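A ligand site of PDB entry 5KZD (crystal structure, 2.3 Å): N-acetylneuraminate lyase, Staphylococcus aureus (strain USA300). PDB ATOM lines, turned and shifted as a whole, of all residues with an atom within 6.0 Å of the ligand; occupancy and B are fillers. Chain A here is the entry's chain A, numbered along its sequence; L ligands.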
ATOM      1  N   ALA A  11      -1.255  -6.925  -3.703  1.00  0.00           N
ATOM      2  CA  ALA A  11       0.127  -6.537  -3.501  1.00  0.00           C
ATOM      3  C   ALA A  11       0.119  -5.028  -3.448  1.00  0.00           C
ATOM      4  O   ALA A  11      -0.010  -4.363  -4.476  1.00  0.00           O
ATOM      5  CB  ALA A  11       1.031  -7.060  -4.609  1.00  0.00           C
ATOM      6  N   LEU A  12       0.214  -4.489  -2.239  1.00  0.00           N
ATOM      7  CA  LEU A  12      -0.026  -3.065  -1.981  1.00  0.00           C
ATOM      8  C   LEU A  12       0.907  -2.106  -2.749  1.00  0.00           C
ATOM      9  O   LEU A  12       2.136  -2.114  -2.541  1.00  0.00           O
ATOM     10  CB  LEU A  12       0.109  -2.811  -0.485  1.00  0.00           C
ATOM     11  CG  LEU A  12      -0.184  -1.379  -0.046  1.00  0.00           C
ATOM     12  CD1 LEU A  12      -1.660  -1.063  -0.300  1.00  0.00           C
ATOM     13  CD2 LEU A  12       0.178  -1.197   1.411  1.00  0.00           C
ATOM     14  N   TYR A  44      -0.835  -7.671   0.973  1.00  0.00           N
ATOM     15  CA  TYR A  44       0.545  -8.166   0.973  1.00  0.00           C
ATOM     16  C   TYR A  44       1.437  -6.931   0.890  1.00  0.00           C
ATOM     17  O   TYR A  44       1.467  -6.264  -0.146  1.00  0.00           O
ATOM     18  CB  TYR A  44       0.777  -9.122  -0.204  1.00  0.00           C
ATOM     19  CG  TYR A  44       2.107  -9.845  -0.221  1.00  0.00           C
ATOM     20  CD1 TYR A  44       2.272 -11.048   0.466  1.00  0.00           C
ATOM     21  CD2 TYR A  44       3.179  -9.347  -0.933  1.00  0.00           C
ATOM     22  CE1 TYR A  44       3.482 -11.723   0.445  1.00  0.00           C
ATOM     23  CE2 TYR A  44       4.405 -10.011  -0.966  1.00  0.00           C
ATOM     24  CZ  TYR A  44       4.545 -11.196  -0.277  1.00  0.00           C
ATOM     25  OH  TYR A  44       5.756 -11.841  -0.311  1.00  0.00           O
ATOM     26  N   ASN A  46       4.870  -4.389   1.259  1.00  0.00           N
ATOM     27  CA  ASN A  46       6.303  -4.274   0.948  1.00  0.00           C
ATOM     28  C   ASN A  46       6.792  -5.438   0.092  1.00  0.00           C
ATOM     29  O   ASN A  46       7.940  -5.842   0.210  1.00  0.00           O
ATOM     30  CB  ASN A  46       7.172  -4.178   2.212  1.00  0.00           C
ATOM     31  CG  ASN A  46       7.129  -2.805   2.854  1.00  0.00           C
ATOM     32  OD1 ASN A  46       6.940  -1.793   2.181  1.00  0.00           O
ATOM     33  ND2 ASN A  46       7.325  -2.764   4.147  1.00  0.00           N
ATOM     34  N   GLY A  47       5.912  -5.964  -0.745  1.00  0.00           N
ATOM     35  CA  GLY A  47       6.363  -6.852  -1.798  1.00  0.00           C
ATOM     36  C   GLY A  47       6.908  -5.981  -2.922  1.00  0.00           C
ATOM     37  O   GLY A  47       6.915  -4.755  -2.824  1.00  0.00           O
ATOM     38  N   SER A  48       7.320  -6.619  -4.014  1.00  0.00           N
ATOM     39  CA  SER A  48       7.943  -5.897  -5.116  1.00  0.00           C
ATOM     40  C   SER A  48       6.980  -4.953  -5.836  1.00  0.00           C
ATOM     41  O   SER A  48       7.425  -4.052  -6.518  1.00  0.00           O
ATOM     42  CB  SER A  48       8.563  -6.876  -6.110  1.00  0.00           C
ATOM     43  OG  SER A  48       7.781  -8.051  -6.226  1.00  0.00           O
ATOM     44  N   SER A  49       5.681  -5.142  -5.664  1.00  0.00           N
ATOM     45  CA  SER A  49       4.702  -4.232  -6.296  1.00  0.00           C
ATOM     46  C   SER A  49       4.642  -2.889  -5.596  1.00  0.00           C
ATOM     47  O   SER A  49       4.245  -1.893  -6.197  1.00  0.00           O
ATOM     48  CB  SER A  49       3.303  -4.845  -6.307  1.00  0.00           C
ATOM     49  OG  SER A  49       3.239  -6.014  -7.109  1.00  0.00           O
ATOM     50  N   GLY A  50       5.008  -2.866  -4.323  1.00  0.00           N
ATOM     51  CA  GLY A  50       5.073  -1.626  -3.571  1.00  0.00           C
ATOM     52  C   GLY A  50       6.465  -1.026  -3.641  1.00  0.00           C
ATOM     53  O   GLY A  50       6.826  -0.224  -2.778  1.00  0.00           O
ATOM     54  N   GLN A  80       6.119  -8.597   3.828  1.00  0.00           N
ATOM     55  CA  GLN A  80       7.334  -8.948   3.111  1.00  0.00           C
ATOM     56  C   GLN A  80       8.519  -8.243   3.696  1.00  0.00           C
ATOM     57  O   GLN A  80       8.695  -7.043   3.538  1.00  0.00           O
ATOM     58  CB  GLN A  80       7.239  -8.514   1.685  1.00  0.00           C
ATOM     59  CG  GLN A  80       8.166  -9.041   0.575  1.00  0.00           C
ATOM     60  CD  GLN A  80       9.687  -9.168   0.868  1.00  0.00           C
ATOM     61  OE1 GLN A  80      10.137  -9.240   2.004  1.00  0.00           O
ATOM     62  NE2 GLN A  80      10.455  -8.881  -0.148  1.00  0.00           N
ATOM     63  N   TYR A 137       9.440 -17.698  -0.843  1.00  0.00           N
ATOM     64  CA  TYR A 137       9.328 -17.451  -2.288  1.00  0.00           C
ATOM     65  C   TYR A 137      10.637 -16.951  -2.917  1.00  0.00           C
ATOM     66  O   TYR A 137      11.463 -16.343  -2.237  1.00  0.00           O
ATOM     67  CB  TYR A 137       8.212 -16.441  -2.573  1.00  0.00           C
ATOM     68  CG  TYR A 137       8.599 -14.990  -2.593  1.00  0.00           C
ATOM     69  CD1 TYR A 137       8.604 -14.230  -1.428  1.00  0.00           C
ATOM     70  CD2 TYR A 137       8.876 -14.349  -3.794  1.00  0.00           C
ATOM     71  CE1 TYR A 137       8.918 -12.881  -1.463  1.00  0.00           C
ATOM     72  CE2 TYR A 137       9.186 -13.013  -3.844  1.00  0.00           C
ATOM     73  CZ  TYR A 137       9.205 -12.279  -2.685  1.00  0.00           C
ATOM     74  OH  TYR A 137       9.522 -10.945  -2.776  1.00  0.00           O
ATOM     75  N   LYS A 165       4.707 -18.250  -1.506  1.00  0.00           N
ATOM     76  CA  LYS A 165       4.137 -17.421  -2.559  1.00  0.00           C
ATOM     77  C   LYS A 165       4.741 -17.924  -3.853  1.00  0.00           C
ATOM     78  O   LYS A 165       5.916 -17.734  -4.122  1.00  0.00           O
ATOM     79  CB  LYS A 165       4.426 -15.923  -2.356  1.00  0.00           C
ATOM     80  CG  LYS A 165       3.929 -15.024  -3.501  1.00  0.00           C
ATOM     81  CD  LYS A 165       4.308 -13.546  -3.327  1.00  0.00           C
ATOM     82  CE  LYS A 165       5.658 -13.219  -3.959  1.00  0.00           C
ATOM     83  NZ  LYS A 165       6.270 -11.918  -3.512  1.00  0.00           N
ATOM     84  N   THR A 167       5.497 -18.153  -7.636  1.00  0.00           N
ATOM     85  CA  THR A 167       5.518 -17.173  -8.718  1.00  0.00           C
ATOM     86  C   THR A 167       6.109 -17.711 -10.033  1.00  0.00           C
ATOM     87  O   THR A 167       6.004 -17.064 -11.063  1.00  0.00           O
ATOM     88  CB  THR A 167       6.309 -15.932  -8.284  1.00  0.00           C
ATOM     89  OG1 THR A 167       7.571 -16.331  -7.747  1.00  0.00           O
ATOM     90  CG2 THR A 167       5.523 -15.193  -7.216  1.00  0.00           C
ATOM     91  N   SER A 188      -0.659 -18.089  -5.209  1.00  0.00           N
ATOM     92  CA  SER A 188      -0.034 -17.864  -6.492  1.00  0.00           C
ATOM     93  C   SER A 188       0.226 -16.371  -6.658  1.00  0.00           C
ATOM     94  O   SER A 188      -0.494 -15.552  -6.097  1.00  0.00           O
ATOM     95  CB  SER A 188      -0.900 -18.412  -7.624  1.00  0.00           C
ATOM     96  OG  SER A 188      -2.259 -18.348  -7.285  1.00  0.00           O
ATOM     97  N   GLY A 189       1.273 -16.052  -7.409  1.00  0.00           N
ATOM     98  CA  GLY A 189       1.642 -14.665  -7.653  1.00  0.00           C
ATOM     99  C   GLY A 189       1.429 -14.155  -9.067  1.00  0.00           C
ATOM    100  O   GLY A 189       1.723 -12.999  -9.334  1.00  0.00           O
ATOM    101  N   PHE A 190       0.919 -14.989  -9.966  1.00  0.00           N
ATOM    102  CA  PHE A 190       0.716 -14.630 -11.370  1.00  0.00           C
ATOM    103  C   PHE A 190      -0.771 -14.377 -11.715  1.00  0.00           C
ATOM    104  O   PHE A 190      -1.550 -15.323 -11.886  1.00  0.00           O
ATOM    105  CB  PHE A 190       1.312 -15.705 -12.300  1.00  0.00           C
ATOM    106  CG  PHE A 190       1.261 -17.112 -11.739  1.00  0.00           C
ATOM    107  CD1 PHE A 190       0.065 -17.794 -11.650  1.00  0.00           C
ATOM    108  CD2 PHE A 190       2.420 -17.742 -11.327  1.00  0.00           C
ATOM    109  CE1 PHE A 190       0.009 -19.089 -11.134  1.00  0.00           C
ATOM    110  CE2 PHE A 190       2.357 -19.052 -10.809  1.00  0.00           C
ATOM    111  CZ  PHE A 190       1.164 -19.711 -10.728  1.00  0.00           C
ATOM    112  N   ASP A 191      -1.164 -13.113 -11.824  1.00  0.00           N
ATOM    113  CA  ASP A 191      -2.571 -12.747 -11.988  1.00  0.00           C
ATOM    114  C   ASP A 191      -3.138 -13.277 -13.295  1.00  0.00           C
ATOM    115  O   ASP A 191      -4.314 -13.643 -13.371  1.00  0.00           O
ATOM    116  CB  ASP A 191      -2.754 -11.217 -11.958  1.00  0.00           C
ATOM    117  CG  ASP A 191      -2.005 -10.563 -10.827  1.00  0.00           C
ATOM    118  OD1 ASP A 191      -1.230 -11.277 -10.151  1.00  0.00           O
ATOM    119  OD2 ASP A 191      -2.175  -9.338 -10.623  1.00  0.00           O
ATOM    120  N   GLU A 192      -2.302 -13.316 -14.319  1.00  0.00           N
ATOM    121  CA  GLU A 192      -2.776 -13.650 -15.658  1.00  0.00           C
ATOM    122  C   GLU A 192      -3.018 -15.145 -15.764  1.00  0.00           C
ATOM    123  O   GLU A 192      -3.407 -15.633 -16.834  1.00  0.00           O
ATOM    124  CB  GLU A 192      -1.792 -13.181 -16.732  1.00  0.00           C
ATOM    125  CG  GLU A 192      -0.356 -13.666 -16.495  1.00  0.00           C
ATOM    126  CD  GLU A 192       0.442 -12.719 -15.610  1.00  0.00           C
ATOM    127  OE1 GLU A 192       0.118 -12.562 -14.405  1.00  0.00           O
ATOM    128  OE2 GLU A 192       1.407 -12.115 -16.122  1.00  0.00           O
ATOM    129  N   ILE A 206      -1.862 -13.593  -4.598  1.00  0.00           N
ATOM    130  CA  ILE A 206      -1.301 -12.297  -4.231  1.00  0.00           C
ATOM    131  C   ILE A 206      -0.998 -11.584  -5.529  1.00  0.00           C
ATOM    132  O   ILE A 206      -0.257 -12.112  -6.354  1.00  0.00           O
ATOM    133  CB  ILE A 206      -0.024 -12.459  -3.420  1.00  0.00           C
ATOM    134  CG1 ILE A 206      -0.356 -13.007  -2.033  1.00  0.00           C
ATOM    135  CG2 ILE A 206       0.721 -11.149  -3.336  1.00  0.00           C
ATOM    136  CD1 ILE A 206       0.861 -13.525  -1.326  1.00  0.00           C
ATOM    137  N   GLY A 207      -1.575 -10.406  -5.739  1.00  0.00           N
ATOM    138  CA  GLY A 207      -1.442  -9.774  -7.037  1.00  0.00           C
ATOM    139  C   GLY A 207      -1.479  -8.254  -7.056  1.00  0.00           C
ATOM    140  O   GLY A 207      -2.236  -7.639  -6.318  1.00  0.00           O
ATOM    141  N   SER A 208      -0.669  -7.653  -7.926  1.00  0.00           N
ATOM    142  CA  SER A 208      -0.650  -6.202  -8.032  1.00  0.00           C
ATOM    143  C   SER A 208      -1.908  -5.683  -8.731  1.00  0.00           C
ATOM    144  O   SER A 208      -2.409  -4.621  -8.392  1.00  0.00           O
ATOM    145  CB  SER A 208       0.600  -5.720  -8.768  1.00  0.00           C
ATOM    146  OG  SER A 208       0.568  -6.139 -10.124  1.00  0.00           O
ATOM    147  N   THR A 209      -2.410  -6.427  -9.711  1.00  0.00           N
ATOM    148  CA  THR A 209      -3.539  -5.922 -10.506  1.00  0.00           C
ATOM    149  C   THR A 209      -4.870  -6.031  -9.747  1.00  0.00           C
ATOM    150  O   THR A 209      -5.863  -5.376 -10.108  1.00  0.00           O
ATOM    151  CB  THR A 209      -3.669  -6.633 -11.893  1.00  0.00           C
ATOM    152  OG1 THR A 209      -3.998  -8.008 -11.709  1.00  0.00           O
ATOM    153  CG2 THR A 209      -2.392  -6.502 -12.728  1.00  0.00           C
ATOM    154  N   TYR A 210      -4.897  -6.857  -8.692  1.00  0.00           N
ATOM    155  CA  TYR A 210      -6.090  -7.006  -7.845  1.00  0.00           C
ATOM    156  C   TYR A 210      -6.431  -5.681  -7.151  1.00  0.00           C
ATOM    157  O   TYR A 210      -7.555  -5.491  -6.675  1.00  0.00           O
ATOM    158  CB  TYR A 210      -5.904  -8.118  -6.797  1.00  0.00           C
ATOM    159  CG  TYR A 210      -5.538  -9.460  -7.372  1.00  0.00           C
ATOM    160  CD1 TYR A 210      -5.895  -9.811  -8.667  1.00  0.00           C
ATOM    161  CD2 TYR A 210      -4.809 -10.375  -6.629  1.00  0.00           C
ATOM    162  CE1 TYR A 210      -5.551 -11.040  -9.189  1.00  0.00           C
ATOM    163  CE2 TYR A 210      -4.464 -11.598  -7.144  1.00  0.00           C
ATOM    164  CZ  TYR A 210      -4.830 -11.929  -8.426  1.00  0.00           C
ATOM    165  OH  TYR A 210      -4.462 -13.149  -8.935  1.00  0.00           O
ATOM    166  N   ILE A 243      -4.425  -6.898 -17.902  1.00  0.00           N
ATOM    167  CA  ILE A 243      -3.058  -7.134 -17.465  1.00  0.00           C
ATOM    168  C   ILE A 243      -2.072  -6.918 -18.600  1.00  0.00           C
ATOM    169  O   ILE A 243      -1.022  -6.355 -18.388  1.00  0.00           O
ATOM    170  CB  ILE A 243      -2.894  -8.563 -16.890  1.00  0.00           C
ATOM    171  CG1 ILE A 243      -3.717  -8.702 -15.600  1.00  0.00           C
ATOM    172  CG2 ILE A 243      -1.447  -8.835 -16.546  1.00  0.00           C
ATOM    173  CD1 ILE A 243      -3.838 -10.104 -15.164  1.00  0.00           C
ATOM    174  N   LEU A 247       0.789  -4.023 -18.573  1.00  0.00           N
ATOM    175  CA  LEU A 247       2.203  -4.379 -18.677  1.00  0.00           C
ATOM    176  C   LEU A 247       2.837  -3.567 -19.794  1.00  0.00           C
ATOM    177  O   LEU A 247       3.967  -3.111 -19.680  1.00  0.00           O
ATOM    178  CB  LEU A 247       2.393  -5.886 -18.906  1.00  0.00           C
ATOM    179  CG  LEU A 247       2.171  -6.807 -17.697  1.00  0.00           C
ATOM    180  CD1 LEU A 247       1.890  -8.222 -18.126  1.00  0.00           C
ATOM    181  CD2 LEU A 247       3.390  -6.768 -16.769  1.00  0.00           C
ATOM    182  N   ILE A 251       3.712  -1.339 -15.509  1.00  0.00           N
ATOM    183  CA  ILE A 251       2.586  -1.849 -14.746  1.00  0.00           C
ATOM    184  C   ILE A 251       2.299  -1.018 -13.487  1.00  0.00           C
ATOM    185  O   ILE A 251       1.143  -0.663 -13.247  1.00  0.00           O
ATOM    186  CB  ILE A 251       2.779  -3.356 -14.392  1.00  0.00           C
ATOM    187  CG1 ILE A 251       1.669  -3.848 -13.460  1.00  0.00           C
ATOM    188  CG2 ILE A 251       4.147  -3.625 -13.737  1.00  0.00           C
ATOM    189  CD1 ILE A 251       1.340  -5.328 -13.616  1.00  0.00           C
ATOM    190  N   TYR A 252       3.314  -0.683 -12.698  1.00  0.00           N
ATOM    191  CA  TYR A 252       3.009  -0.014 -11.425  1.00  0.00           C
ATOM    192  C   TYR A 252       2.503   1.411 -11.641  1.00  0.00           C
ATOM    193  O   TYR A 252       1.484   1.777 -11.059  1.00  0.00           O
ATOM    194  CB  TYR A 252       4.204  -0.018 -10.468  1.00  0.00           C
ATOM    195  CG  TYR A 252       4.774  -1.394 -10.228  1.00  0.00           C
ATOM    196  CD1 TYR A 252       3.937  -2.499 -10.083  1.00  0.00           C
ATOM    197  CD2 TYR A 252       6.150  -1.603 -10.157  1.00  0.00           C
ATOM    198  CE1 TYR A 252       4.454  -3.778  -9.878  1.00  0.00           C
ATOM    199  CE2 TYR A 252       6.679  -2.873  -9.949  1.00  0.00           C
ATOM    200  CZ  TYR A 252       5.836  -3.957  -9.808  1.00  0.00           C
ATOM    201  OH  TYR A 252       6.368  -5.205  -9.607  1.00  0.00           O
HETATM  202  O1  LIG L   1       5.473  -9.328  -3.905  1.00  0.00           O
HETATM  203  C1  LIG L   1       4.710  -8.890  -4.800  1.00  0.00           C
HETATM  204  O2  LIG L   1       4.285  -7.703  -4.832  1.00  0.00           O
HETATM  205  C2  LIG L   1       4.287  -9.849  -5.876  1.00  0.00           C
HETATM  206  O3  LIG L   1       3.270 -10.728  -5.405  1.00  0.00           O
HETATM  207  C3  LIG L   1       3.799  -9.078  -7.085  1.00  0.00           C
HETATM  208  C4  LIG L   1       2.819  -9.850  -7.966  1.00  0.00           C
HETATM  209  O4  LIG L   1       2.977 -11.276  -7.867  1.00  0.00           O
HETATM  210  C5  LIG L   1       2.954  -9.444  -9.429  1.00  0.00           C
HETATM  211  N1  LIG L   1       4.349  -9.681  -9.784  1.00  0.00           N
HETATM  212  C6  LIG L   1       5.223  -8.651  -9.926  1.00  0.00           C
HETATM  213  C7  LIG L   1       6.672  -8.984 -10.125  1.00  0.00           C
HETATM  214  O5  LIG L   1       4.888  -7.469  -9.865  1.00  0.00           O
HETATM  215  C8  LIG L   1       1.827 -10.179 -10.190  1.00  0.00           C
HETATM  216  O6  LIG L   1       0.627  -9.837  -9.495  1.00  0.00           O
HETATM  217  C9  LIG L   1       1.522  -9.884 -11.665  1.00  0.00           C
HETATM  218  O7  LIG L   1       1.050 -11.030 -12.414  1.00  0.00           O
HETATM  219  C10 LIG L   1       2.699  -9.245 -12.348  1.00  0.00           C
HETATM  220  O8  LIG L   1       2.485  -7.856 -12.064  1.00  0.00           O
HETATM  221  C11 LIG L   1       2.759  -9.602 -13.834  1.00  0.00           C
HETATM  222  O9  LIG L   1       1.458  -9.395 -14.367  1.00  0.00           O
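The side-chain amino group (NZ) of Lys 165 sits at hydrogen-bond distance from the side-chain hydroxyl (OH) of Tyr 44, at 3.2 Å. The side-chain hydroxyl (OH) of Tyr 252 lies within hydrogen-bond range of the backbone carbonyl oxygen (O) of Ser 48 (3.5 Å). The backbone carbonyl oxygen (O) of Tyr 44 lies within hydrogen-bond range of the backbone NH (N) of Leu 12. N of Ala 11 is in hydrogen-bond range of O of Gly 207. The side-chain carboxylate of Asp 191 is in hydrogen-bond range of the side-chain hydroxyl of Thr 209, 2.5 Å away. N of Ile 206 is in hydrogen-bond range of O of Ser 188, 2.8 Å away. The side-chain amino group (NZ) of Lys 165 sits close to the side-chain hydroxyl (OH) of Tyr 137 (3.5 Å).
O2 of the ligand sits at hydrogen-bond distance from OG of Ser 49 (3.0 Å). The side-chain amino group (NZ) of Lys 165 lies within salt-bridge range of an oxygen (O1) of the ligand (2.7 Å). N of Asp 191 is in hydrogen-bond range of O7 of the ligand. The side-chain hydroxyl of Ser 208 sits at hydrogen-bond distance from an oxygen (O8) of the ligand, 3.2 Å away. The backbone carbonyl oxygen (O) of Gly 189 is in hydrogen-bond range of an oxygen (O4) of the ligand, at 2.6 Å. OE1 of Glu 192 is in hydrogen-bond range of O7 of the ligand, 2.7 Å away. The backbone NH of Ser 49 is in hydrogen-bond range of an oxygen (O2) of the ligand, 3.0 Å away. The backbone NH (N) of Ser 48 sits at hydrogen-bond distance from an oxygen (O1) of the ligand (3.3 Å). OH of Tyr 252 sits at hydrogen-bond distance from O5 of the ligand, 2.7 Å away. O6 of the ligand is in hydrogen-bond range of N of Ser 208. OD1 of Asp 191 lies within hydrogen-bond range of O6 of the ligand (2.4 Å).
Ala 11 touches the ligand. Tyr 44 touches the ligand (CE2 to O1, 3.2 Å). CA of Gly 47 touches O1 of the ligand, 3.4 Å away. Phe 190 touches the ligand. CG2 of Ile 206 touches O3 of the ligand (3.3 Å). Gly 207 touches the ligand. Ile 243 touches the ligand. CD1 of Leu 247 touches O9 of the ligand (3.96 Å). Ile 251 touches the ligand (CD1 to O8, 3.2 Å). Hydrophobic or aromatic side chains that line the ligand: Ala 11, Tyr 44, Ile 206, Ile 243, Leu 247, Ile 251 and Tyr 252. 17 residues have an atom within 4 Å of the ligand: Ala 11, Tyr 44, Gly 47, Ser 48, Ser 49, Lys 165, Gly 189, Phe 190, Asp 191, Glu 192, Ile 206, Gly 207, Ser 208, Ile 243, Leu 247, Ile 251 and Tyr 252.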
